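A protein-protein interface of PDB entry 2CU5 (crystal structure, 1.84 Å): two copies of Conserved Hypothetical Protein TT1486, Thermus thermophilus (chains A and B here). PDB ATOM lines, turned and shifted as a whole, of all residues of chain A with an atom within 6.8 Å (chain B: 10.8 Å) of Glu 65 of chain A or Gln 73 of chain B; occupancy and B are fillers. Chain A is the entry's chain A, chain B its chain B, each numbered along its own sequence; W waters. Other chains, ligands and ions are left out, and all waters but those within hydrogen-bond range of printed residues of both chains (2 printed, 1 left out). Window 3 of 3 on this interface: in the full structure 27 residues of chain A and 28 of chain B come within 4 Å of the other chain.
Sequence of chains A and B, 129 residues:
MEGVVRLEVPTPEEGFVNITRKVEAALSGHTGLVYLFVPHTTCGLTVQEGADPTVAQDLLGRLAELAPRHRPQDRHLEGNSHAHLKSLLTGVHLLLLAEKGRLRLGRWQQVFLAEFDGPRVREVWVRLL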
ATOM      1  N   ASP A  58     -19.715 -10.666  -6.866  1.00  0.00           N
ATOM      2  CA  ASP A  58     -19.126 -11.930  -6.442  1.00  0.00           C
ATOM      3  C   ASP A  58     -17.598 -11.888  -6.467  1.00  0.00           C
ATOM      4  O   ASP A  58     -16.946 -12.480  -5.605  1.00  0.00           O
ATOM      5  CB  ASP A  58     -19.637 -13.084  -7.312  1.00  0.00           C
ATOM      6  CG  ASP A  58     -21.103 -13.401  -7.063  1.00  0.00           C
ATOM      7  OD1 ASP A  58     -21.706 -12.777  -6.169  1.00  0.00           O
ATOM      8  OD2 ASP A  58     -21.654 -14.280  -7.759  1.00  0.00           O
ATOM      9  N   LEU A  60     -15.585  -9.307  -5.879  1.00  0.00           N
ATOM     10  CA  LEU A  60     -15.131  -8.582  -4.698  1.00  0.00           C
ATOM     11  C   LEU A  60     -15.369  -9.391  -3.424  1.00  0.00           C
ATOM     12  O   LEU A  60     -14.542  -9.390  -2.510  1.00  0.00           O
ATOM     13  CB  LEU A  60     -15.856  -7.238  -4.592  1.00  0.00           C
ATOM     14  CG  LEU A  60     -15.468  -6.179  -5.631  1.00  0.00           C
ATOM     15  CD1 LEU A  60     -16.393  -4.983  -5.521  1.00  0.00           C
ATOM     16  CD2 LEU A  60     -14.020  -5.765  -5.417  1.00  0.00           C
ATOM     17  N   GLY A  61     -16.513 -10.063  -3.366  1.00  0.00           N
ATOM     18  CA  GLY A  61     -16.836 -10.870  -2.205  1.00  0.00           C
ATOM     19  C   GLY A  61     -15.846 -12.005  -2.045  1.00  0.00           C
ATOM     20  O   GLY A  61     -15.351 -12.262  -0.950  1.00  0.00           O
ATOM     21  N   ARG A  62     -15.538 -12.678  -3.148  1.00  0.00           N
ATOM     22  CA  ARG A  62     -14.597 -13.789  -3.117  1.00  0.00           C
ATOM     23  C   ARG A  62     -13.165 -13.317  -2.861  1.00  0.00           C
ATOM     24  O   ARG A  62     -12.402 -13.980  -2.161  1.00  0.00           O
ATOM     25  CB  ARG A  62     -14.683 -14.579  -4.423  1.00  0.00           C
ATOM     26  CG  ARG A  62     -15.954 -15.422  -4.551  1.00  0.00           C
ATOM     27  CD  ARG A  62     -16.094 -15.963  -5.965  1.00  0.00           C
ATOM     28  NE  ARG A  62     -17.219 -16.879  -6.156  1.00  0.00           N
ATOM     29  CZ  ARG A  62     -17.125 -18.205  -6.114  1.00  0.00           C
ATOM     30  NH1 ARG A  62     -15.953 -18.785  -5.872  1.00  0.00           N
ATOM     31  NH2 ARG A  62     -18.193 -18.956  -6.366  1.00  0.00           N
ATOM     32  N   LEU A  63     -12.792 -12.172  -3.424  1.00  0.00           N
ATOM     33  CA  LEU A  63     -11.446 -11.647  -3.204  1.00  0.00           C
ATOM     34  C   LEU A  63     -11.235 -11.285  -1.735  1.00  0.00           C
ATOM     35  O   LEU A  63     -10.118 -11.367  -1.216  1.00  0.00           O
ATOM     36  CB  LEU A  63     -11.204 -10.409  -4.073  1.00  0.00           C
ATOM     37  CG  LEU A  63     -10.896 -10.673  -5.545  1.00  0.00           C
ATOM     38  CD1 LEU A  63     -10.885  -9.347  -6.291  1.00  0.00           C
ATOM     39  CD2 LEU A  63      -9.546 -11.374  -5.682  1.00  0.00           C
ATOM     40  N   ALA A  64     -12.307 -10.879  -1.066  1.00  0.00           N
ATOM     41  CA  ALA A  64     -12.216 -10.519   0.342  1.00  0.00           C
ATOM     42  C   ALA A  64     -11.952 -11.773   1.175  1.00  0.00           C
ATOM     43  O   ALA A  64     -11.274 -11.719   2.205  1.00  0.00           O
ATOM     44  CB  ALA A  64     -13.504  -9.834   0.796  1.00  0.00           C
ATOM     45  N   GLU A  65     -12.482 -12.903   0.721  1.00  0.00           N
ATOM     46  CA  GLU A  65     -12.290 -14.163   1.426  1.00  0.00           C
ATOM     47  C   GLU A  65     -10.860 -14.647   1.212  1.00  0.00           C
ATOM     48  O   GLU A  65     -10.250 -15.234   2.105  1.00  0.00           O
ATOM     49  CB  GLU A  65     -13.309 -15.205   0.933  1.00  0.00           C
ATOM     50  CG  GLU A  65     -14.764 -14.736   1.071  1.00  0.00           C
ATOM     51  CD  GLU A  65     -15.785 -15.784   0.659  1.00  0.00           C
ATOM     52  OE1 GLU A  65     -15.604 -16.413  -0.401  1.00  0.00           O
ATOM     53  OE2 GLU A  65     -16.780 -15.971   1.390  1.00  0.00           O
ATOM     54  N   LEU A  66     -10.314 -14.377   0.030  1.00  0.00           N
ATOM     55  CA  LEU A  66      -8.947 -14.779  -0.272  1.00  0.00           C
ATOM     56  C   LEU A  66      -7.954 -13.824   0.384  1.00  0.00           C
ATOM     57  O   LEU A  66      -6.864 -14.228   0.797  1.00  0.00           O
ATOM     58  CB  LEU A  66      -8.723 -14.800  -1.786  1.00  0.00           C
ATOM     59  CG  LEU A  66      -9.549 -15.822  -2.573  1.00  0.00           C
ATOM     60  CD1 LEU A  66      -9.187 -15.744  -4.037  1.00  0.00           C
ATOM     61  CD2 LEU A  66      -9.284 -17.219  -2.034  1.00  0.00           C
ATOM     62  N   ALA A  67      -8.340 -12.558   0.486  1.00  0.00           N
ATOM     63  CA  ALA A  67      -7.489 -11.537   1.086  1.00  0.00           C
ATOM     64  C   ALA A  67      -8.260 -10.729   2.123  1.00  0.00           C
ATOM     65  O   ALA A  67      -8.646  -9.592   1.875  1.00  0.00           O
ATOM     66  CB  ALA A  67      -6.945 -10.609  -0.005  1.00  0.00           C
ATOM     67  N   PRO A  68      -8.508 -11.316   3.304  1.00  0.00           N
ATOM     68  CA  PRO A  68      -9.245 -10.592   4.346  1.00  0.00           C
ATOM     69  C   PRO A  68      -8.468  -9.394   4.879  1.00  0.00           C
ATOM     70  O   PRO A  68      -7.243  -9.426   4.963  1.00  0.00           O
ATOM     71  CB  PRO A  68      -9.473 -11.659   5.415  1.00  0.00           C
ATOM     72  CG  PRO A  68      -8.264 -12.545   5.258  1.00  0.00           C
ATOM     73  CD  PRO A  68      -8.142 -12.669   3.757  1.00  0.00           C
ATOM     74  N   LYS A  86      -4.558  -8.139  -3.237  1.00  0.00           N
ATOM     75  CA  LYS A  86      -5.553  -8.140  -4.301  1.00  0.00           C
ATOM     76  C   LYS A  86      -4.971  -7.508  -5.564  1.00  0.00           C
ATOM     77  O   LYS A  86      -5.269  -7.941  -6.681  1.00  0.00           O
ATOM     78  CB  LYS A  86      -6.804  -7.390  -3.863  1.00  0.00           C
ATOM     79  CG  LYS A  86      -7.544  -8.074  -2.724  1.00  0.00           C
ATOM     80  CD  LYS A  86      -8.706  -7.241  -2.256  1.00  0.00           C
ATOM     81  CE  LYS A  86      -9.411  -7.902  -1.073  1.00  0.00           C
ATOM     82  NZ  LYS A  86     -10.456  -6.992  -0.553  1.00  0.00           N
ATOM     83  N   LEU B  63      -6.956 -24.196  -7.654  1.00  0.00           N
ATOM     84  CA  LEU B  63      -7.773 -23.050  -8.042  1.00  0.00           C
ATOM     85  C   LEU B  63      -9.232 -23.305  -7.670  1.00  0.00           C
ATOM     86  O   LEU B  63      -9.948 -22.386  -7.275  1.00  0.00           O
ATOM     87  CB  LEU B  63      -7.643 -22.774  -9.544  1.00  0.00           C
ATOM     88  CG  LEU B  63      -6.357 -22.053  -9.954  1.00  0.00           C
ATOM     89  CD1 LEU B  63      -6.255 -22.009 -11.478  1.00  0.00           C
ATOM     90  CD2 LEU B  63      -6.351 -20.641  -9.377  1.00  0.00           C
ATOM     91  N   ALA B  64      -9.672 -24.556  -7.778  1.00  0.00           N
ATOM     92  CA  ALA B  64     -11.053 -24.887  -7.431  1.00  0.00           C
ATOM     93  C   ALA B  64     -11.265 -24.686  -5.927  1.00  0.00           C
ATOM     94  O   ALA B  64     -12.349 -24.301  -5.487  1.00  0.00           O
ATOM     95  CB  ALA B  64     -11.374 -26.328  -7.833  1.00  0.00           C
ATOM     96  N   GLU B  65     -10.221 -24.935  -5.144  1.00  0.00           N
ATOM     97  CA  GLU B  65     -10.299 -24.757  -3.695  1.00  0.00           C
ATOM     98  C   GLU B  65     -10.331 -23.267  -3.355  1.00  0.00           C
ATOM     99  O   GLU B  65     -11.029 -22.836  -2.432  1.00  0.00           O
ATOM    100  CB  GLU B  65      -9.112 -25.446  -3.022  1.00  0.00           C
ATOM    101  CG  GLU B  65      -9.244 -26.969  -3.015  1.00  0.00           C
ATOM    102  CD  GLU B  65      -8.018 -27.674  -2.481  1.00  0.00           C
ATOM    103  OE1 GLU B  65      -7.246 -27.044  -1.730  1.00  0.00           O
ATOM    104  OE2 GLU B  65      -7.836 -28.866  -2.803  1.00  0.00           O
ATOM    105  N   LEU B  66      -9.587 -22.472  -4.114  1.00  0.00           N
ATOM    106  CA  LEU B  66      -9.563 -21.030  -3.893  1.00  0.00           C
ATOM    107  C   LEU B  66     -10.838 -20.387  -4.428  1.00  0.00           C
ATOM    108  O   LEU B  66     -11.313 -19.384  -3.892  1.00  0.00           O
ATOM    109  CB  LEU B  66      -8.343 -20.410  -4.582  1.00  0.00           C
ATOM    110  CG  LEU B  66      -7.001 -20.769  -3.935  1.00  0.00           C
ATOM    111  CD1 LEU B  66      -5.852 -20.322  -4.828  1.00  0.00           C
ATOM    112  CD2 LEU B  66      -6.914 -20.119  -2.555  1.00  0.00           C
ATOM    113  N   ALA B  67     -11.396 -20.973  -5.482  1.00  0.00           N
ATOM    114  CA  ALA B  67     -12.608 -20.441  -6.092  1.00  0.00           C
ATOM    115  C   ALA B  67     -13.638 -21.546  -6.277  1.00  0.00           C
ATOM    116  O   ALA B  67     -13.845 -22.034  -7.385  1.00  0.00           O
ATOM    117  CB  ALA B  67     -12.272 -19.792  -7.446  1.00  0.00           C
ATOM    118  N   PRO B  68     -14.301 -21.954  -5.181  1.00  0.00           N
ATOM    119  CA  PRO B  68     -15.320 -23.010  -5.193  1.00  0.00           C
ATOM    120  C   PRO B  68     -16.475 -22.702  -6.137  1.00  0.00           C
ATOM    121  O   PRO B  68     -16.922 -21.557  -6.228  1.00  0.00           O
ATOM    122  CB  PRO B  68     -15.782 -23.061  -3.741  1.00  0.00           C
ATOM    123  CG  PRO B  68     -14.576 -22.617  -2.982  1.00  0.00           C
ATOM    124  CD  PRO B  68     -14.077 -21.461  -3.812  1.00  0.00           C
ATOM    125  N   ARG B  69     -16.962 -23.729  -6.830  1.00  0.00           N
ATOM    126  CA  ARG B  69     -18.073 -23.568  -7.760  1.00  0.00           C
ATOM    127  C   ARG B  69     -19.364 -23.192  -7.053  1.00  0.00           C
ATOM    128  O   ARG B  69     -20.112 -22.331  -7.516  1.00  0.00           O
ATOM    129  CB  ARG B  69     -18.321 -24.862  -8.539  1.00  0.00           C
ATOM    130  CG  ARG B  69     -17.336 -25.147  -9.640  1.00  0.00           C
ATOM    131  CD  ARG B  69     -17.494 -26.578 -10.129  1.00  0.00           C
ATOM    132  NE  ARG B  69     -16.576 -26.879 -11.224  1.00  0.00           N
ATOM    133  CZ  ARG B  69     -16.762 -26.482 -12.477  1.00  0.00           C
ATOM    134  NH1 ARG B  69     -17.837 -25.772 -12.793  1.00  0.00           N
ATOM    135  NH2 ARG B  69     -15.870 -26.791 -13.412  1.00  0.00           N
ATOM    136  N   HIS B  70     -19.626 -23.851  -5.929  1.00  0.00           N
ATOM    137  CA  HIS B  70     -20.852 -23.607  -5.188  1.00  0.00           C
ATOM    138  C   HIS B  70     -20.606 -22.815  -3.913  1.00  0.00           C
ATOM    139  O   HIS B  70     -20.217 -23.373  -2.887  1.00  0.00           O
ATOM    140  CB  HIS B  70     -21.523 -24.952  -4.891  1.00  0.00           C
ATOM    141  CG  HIS B  70     -21.732 -25.791  -6.115  1.00  0.00           C
ATOM    142  ND1 HIS B  70     -22.600 -25.429  -7.124  1.00  0.00           N
ATOM    143  CD2 HIS B  70     -21.130 -26.931  -6.529  1.00  0.00           C
ATOM    144  CE1 HIS B  70     -22.523 -26.310  -8.106  1.00  0.00           C
ATOM    145  NE2 HIS B  70     -21.637 -27.231  -7.771  1.00  0.00           N
ATOM    146  N   ARG B  71     -20.821 -21.505  -4.003  1.00  0.00           N
ATOM    147  CA  ARG B  71     -20.641 -20.576  -2.884  1.00  0.00           C
ATOM    148  C   ARG B  71     -22.005 -19.974  -2.559  1.00  0.00           C
ATOM    149  O   ARG B  71     -22.596 -19.277  -3.387  1.00  0.00           O
ATOM    150  CB  ARG B  71     -19.650 -19.471  -3.276  1.00  0.00           C
ATOM    151  CG  ARG B  71     -19.506 -18.324  -2.270  1.00  0.00           C
ATOM    152  CD  ARG B  71     -18.336 -17.424  -2.651  1.00  0.00           C
ATOM    153  NE  ARG B  71     -18.184 -16.281  -1.752  1.00  0.00           N
ATOM    154  CZ  ARG B  71     -18.798 -15.113  -1.906  1.00  0.00           C
ATOM    155  NH1 ARG B  71     -18.595 -14.141  -1.026  1.00  0.00           N
ATOM    156  NH2 ARG B  71     -19.601 -14.909  -2.946  1.00  0.00           N
ATOM    157  N   PRO B  72     -22.528 -20.238  -1.349  1.00  0.00           N
ATOM    158  CA  PRO B  72     -23.837 -19.710  -0.955  1.00  0.00           C
ATOM    159  C   PRO B  72     -24.027 -18.206  -1.160  1.00  0.00           C
ATOM    160  O   PRO B  72     -25.083 -17.770  -1.616  1.00  0.00           O
ATOM    161  CB  PRO B  72     -23.940 -20.105   0.522  1.00  0.00           C
ATOM    162  CG  PRO B  72     -23.128 -21.352   0.598  1.00  0.00           C
ATOM    163  CD  PRO B  72     -21.921 -21.001  -0.244  1.00  0.00           C
ATOM    164  N   GLN B  73     -23.001 -17.421  -0.837  1.00  0.00           N
ATOM    165  CA  GLN B  73     -23.075 -15.971  -0.951  1.00  0.00           C
ATOM    166  C   GLN B  73     -23.061 -15.396  -2.364  1.00  0.00           C
ATOM    167  O   GLN B  73     -23.275 -14.194  -2.544  1.00  0.00           O
ATOM    168  CB  GLN B  73     -21.956 -15.323  -0.132  1.00  0.00           C
ATOM    169  CG  GLN B  73     -21.944 -15.746   1.327  1.00  0.00           C
ATOM    170  CD  GLN B  73     -20.982 -16.882   1.596  1.00  0.00           C
ATOM    171  OE1 GLN B  73     -20.975 -17.894   0.890  1.00  0.00           O
ATOM    172  NE2 GLN B  73     -20.160 -16.723   2.628  1.00  0.00           N
ATOM    173  N   ASP B  74     -22.804 -16.239  -3.359  1.00  0.00           N
ATOM    174  CA  ASP B  74     -22.784 -15.788  -4.750  1.00  0.00           C
ATOM    175  C   ASP B  74     -24.142 -15.206  -5.145  1.00  0.00           C
ATOM    176  O   ASP B  74     -25.184 -15.759  -4.802  1.00  0.00           O
ATOM    177  CB  ASP B  74     -22.442 -16.957  -5.684  1.00  0.00           C
ATOM    178  CG  ASP B  74     -20.967 -17.022  -6.033  1.00  0.00           C
ATOM    179  OD1 ASP B  74     -20.166 -16.268  -5.438  1.00  0.00           O
ATOM    180  OD2 ASP B  74     -20.611 -17.832  -6.915  1.00  0.00           O
ATOM    181  N   ARG B  75     -24.118 -14.093  -5.874  1.00  0.00           N
ATOM    182  CA  ARG B  75     -25.342 -13.446  -6.323  1.00  0.00           C
ATOM    183  C   ARG B  75     -25.526 -13.668  -7.823  1.00  0.00           C
ATOM    184  O   ARG B  75     -26.627 -13.509  -8.354  1.00  0.00           O
ATOM    185  CB  ARG B  75     -25.282 -11.953  -5.988  1.00  0.00           C
ATOM    186  CG  ARG B  75     -25.002 -11.708  -4.510  1.00  0.00           C
ATOM    187  CD  ARG B  75     -24.595 -10.275  -4.207  1.00  0.00           C
ATOM    188  NE  ARG B  75     -25.741  -9.402  -3.970  1.00  0.00           N
ATOM    189  CZ  ARG B  75     -25.646  -8.136  -3.574  1.00  0.00           C
ATOM    190  NH1 ARG B  75     -24.453  -7.590  -3.369  1.00  0.00           N
ATOM    191  NH2 ARG B  75     -26.745  -7.414  -3.380  1.00  0.00           N
ATOM    192  N   HIS B  76     -24.441 -14.041  -8.496  1.00  0.00           N
ATOM    193  CA  HIS B  76     -24.461 -14.323  -9.931  1.00  0.00           C
ATOM    194  C   HIS B  76     -25.108 -15.697 -10.086  1.00  0.00           C
ATOM    195  O   HIS B  76     -24.436 -16.729 -10.014  1.00  0.00           O
ATOM    196  CB  HIS B  76     -23.028 -14.331 -10.473  1.00  0.00           C
ATOM    197  CG  HIS B  76     -22.935 -14.487 -11.958  1.00  0.00           C
ATOM    198  ND1 HIS B  76     -23.605 -13.664 -12.838  1.00  0.00           N
ATOM    199  CD2 HIS B  76     -22.217 -15.346 -12.718  1.00  0.00           C
ATOM    200  CE1 HIS B  76     -23.301 -14.009 -14.077  1.00  0.00           C
ATOM    201  NE2 HIS B  76     -22.460 -15.027 -14.032  1.00  0.00           N
ATOM    202  N   LEU B  77     -26.423 -15.690 -10.294  1.00  0.00           N
ATOM    203  CA  LEU B  77     -27.222 -16.906 -10.412  1.00  0.00           C
ATOM    204  C   LEU B  77     -26.818 -17.900 -11.485  1.00  0.00           C
ATOM    205  O   LEU B  77     -27.095 -19.093 -11.357  1.00  0.00           O
ATOM    206  CB  LEU B  77     -28.695 -16.532 -10.596  1.00  0.00           C
ATOM    207  CG  LEU B  77     -29.537 -16.322  -9.334  1.00  0.00           C
ATOM    208  CD1 LEU B  77     -28.738 -15.656  -8.230  1.00  0.00           C
ATOM    209  CD2 LEU B  77     -30.749 -15.492  -9.704  1.00  0.00           C
ATOM    210  N   GLY B  79     -24.177 -19.012 -11.932  1.00  0.00           N
ATOM    211  CA  GLY B  79     -23.298 -19.949 -11.259  1.00  0.00           C
ATOM    212  C   GLY B  79     -21.855 -20.082 -11.695  1.00  0.00           C
ATOM    213  O   GLY B  79     -21.167 -20.989 -11.238  1.00  0.00           O
ATOM    214  N   SER B  81     -19.424 -17.667 -11.295  1.00  0.00           N
ATOM    215  CA  SER B  81     -18.558 -16.650 -10.713  1.00  0.00           C
ATOM    216  C   SER B  81     -17.189 -17.243 -10.390  1.00  0.00           C
ATOM    217  O   SER B  81     -16.183 -16.535 -10.402  1.00  0.00           O
ATOM    218  CB  SER B  81     -19.177 -16.063  -9.450  1.00  0.00           C
ATOM    219  OG  SER B  81     -20.229 -15.187  -9.780  1.00  0.00           O
ATOM    220  N   HIS B  82     -17.147 -18.542 -10.101  1.00  0.00           N
ATOM    221  CA  HIS B  82     -15.874 -19.183  -9.796  1.00  0.00           C
ATOM    222  C   HIS B  82     -14.956 -19.051 -11.006  1.00  0.00           C
ATOM    223  O   HIS B  82     -13.750 -18.849 -10.862  1.00  0.00           O
ATOM    224  CB  HIS B  82     -16.066 -20.671  -9.458  1.00  0.00           C
ATOM    225  CG  HIS B  82     -16.387 -21.536 -10.640  1.00  0.00           C
ATOM    226  ND1 HIS B  82     -17.593 -21.478 -11.307  1.00  0.00           N
ATOM    227  CD2 HIS B  82     -15.659 -22.489 -11.266  1.00  0.00           C
ATOM    228  CE1 HIS B  82     -17.594 -22.360 -12.290  1.00  0.00           C
ATOM    229  NE2 HIS B  82     -16.431 -22.987 -12.288  1.00  0.00           N
ATOM    230  N   LEU B  85     -13.688 -15.470 -11.435  1.00  0.00           N
ATOM    231  CA  LEU B  85     -12.585 -15.219 -10.514  1.00  0.00           C
ATOM    232  C   LEU B  85     -11.293 -15.844 -11.010  1.00  0.00           C
ATOM    233  O   LEU B  85     -10.244 -15.201 -10.992  1.00  0.00           O
ATOM    234  CB  LEU B  85     -12.901 -15.757  -9.115  1.00  0.00           C
ATOM    235  CG  LEU B  85     -11.757 -15.628  -8.097  1.00  0.00           C
ATOM    236  CD1 LEU B  85     -11.330 -14.168  -7.952  1.00  0.00           C
ATOM    237  CD2 LEU B  85     -12.227 -16.168  -6.742  1.00  0.00           C
ATOM    238  N   LEU B  89      -7.799 -13.881 -11.892  1.00  0.00           N
ATOM    239  CA  LEU B  89      -6.550 -14.268 -11.245  1.00  0.00           C
ATOM    240  C   LEU B  89      -5.467 -14.693 -12.235  1.00  0.00           C
ATOM    241  O   LEU B  89      -4.279 -14.493 -11.988  1.00  0.00           O
ATOM    242  CB  LEU B  89      -6.803 -15.417 -10.262  1.00  0.00           C
ATOM    243  CG  LEU B  89      -7.709 -15.113  -9.068  1.00  0.00           C
ATOM    244  CD1 LEU B  89      -7.953 -16.391  -8.279  1.00  0.00           C
ATOM    245  CD2 LEU B  89      -7.068 -14.056  -8.189  1.00  0.00           C
HETATM  246  O   HOH W   1     -13.740 -17.861  -3.994  1.00  0.00           O
HETATM  247  O   HOH W   2     -21.344 -12.221  -3.626  1.00  0.00           O
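Of chain B, only Arg 71 and Gln 73 come within 4 Å of Glu 65 of chain A.
Gln 73 of chain B touches just one residue of chain A: Glu 65 (3.7 Å).
Gly 61 of chain A touches one residue of chain B.
No residue of chain B comes within 4 Å of Ala 64 of chain A.
Printed residues of chain B within 4 Å of Leu 66 of chain A: Leu 66.
No residue of chain B comes within 4 Å of Ala 67 of chain A.
Printed residues of chain A within 4 Å of Asp 74 of chain B: Asp 58 and Arg 62.
Printed residues of chain B within 4 Å of Arg 62 of chain A: Ala 67 (3.6 Å), Pro 68 (2.9 Å), Arg 71 (3.5 Å), Asp 74 (2.7 Å), Ser 81 (3.9 Å), His 82 (3.9 Å) and Leu 85 (3.7 Å).
Pro 72 of chain B touches none of the printed residues of chain A.
The nearest residue of chain A that does not touch Gln 73 of chain B is Asp 58 of chain A (4.2 Å).
The nearest printed residue of chain A that does not touch Asp 74 of chain B is Glu 65 of chain A (6.8 Å).
Of the 20 printed residues of chain B, 11 touch a printed residue of chain A.
Hydrophobic or aromatic side chains of chain B that line the printed part of chain A: Leu 66, Pro 68, His 76 and Leu 85.
Along chain B the printed residues that touch a printed residue of chain A span positions 66 to 85.
Of the 11 printed residues of chain A, 5 touch a printed residue of chain B.
Printed residues of chain A that touch a printed residue of chain B: Asp 58, Gly 61, Arg 62, Glu 65 and Leu 66.
Hydrophobic or aromatic side chains of chain A that line the printed part of chain B: Leu 66.
Among the printed residues, 15 pairs touch across the chains.
Among the printed residues, Asp or Glu carboxylates within 4 Å of a Lys or Arg side-chain nitrogen of the other chain: Arg 62 of chain A with Asp 74 of chain B and Glu 65 of chain A with Arg 71 of chain B.
OD1 of Asp 58 of chain A is in hydrogen-bond range of N of Arg 75 of chain B (2.8 Å).
The backbone NH (N) of His 76 of chain B is in hydrogen-bond range of the side-chain carboxylate (OD2) of Asp 58 of chain A.
OD2 of Asp 58 of chain A lies within hydrogen-bond range of OG of Ser 81 of chain B.
The guanidinium group (NH2) of Arg 62 of chain A lies within hydrogen-bond range of the backbone carbonyl oxygen (O) of Pro 68 of chain B (2.9 Å).
The guanidinium group (NH2) of Arg 62 of chain A is in salt-bridge range of the side-chain carboxylate (OD2) of Asp 74 of chain B (2.7 Å).
NE of Arg 71 of chain B is in salt-bridge range of OE1 of Glu 65 of chain A (2.9 Å).
The side-chain carboxylate (OD1) of Asp 74 of chain B lies close to the side-chain carboxylate (OD2) of Asp 58 of chain A, at 3.4 Å.
Leu 66 of chain B touches its own counterpart, Leu 66 of chain A.
Of the 15 pairs that touch across the chains among the printed residues, 1 has its exchanged pair printed and touching as well.
A ring nitrogen (NE2) of His 82 of chain B sits at hydrogen-bond distance from the guanidinium group of Arg 69 of chain B (3.2 Å).
OD1 of Asp 74 of chain B lies within salt-bridge range of NH2 of Arg 71 of chain B (2.9 Å).
Water W2 lies within hydrogen-bond range of OD1 of Asp 58 of chain A, O of Gln 73 of chain B and NH2 of Arg 71 of chain B.
Water W1 lies within hydrogen-bond range of O of Leu 66 of chain B and NH1 of Arg 62 of chain A.
Among the printed residues, pairs that only touch across the chains: Gly 61 of chain A with Arg 71 of chain B (3.6 Å), Arg 62 of chain A with Ala 67 of chain B (3.6 Å), Arg 62 of chain A with Arg 71 of chain B (3.5 Å), Arg 62 of chain A with Ser 81 of chain B (3.9 Å), Arg 62 of chain A with His 82 of chain B (3.9 Å), Arg 62 of chain A with Leu 85 of chain B (3.7 Å), Glu 65 of chain A with Gln 73 of chain B (3.7 Å) and Leu 66 of chain A with Leu 66 of chain B (3.5 Å).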
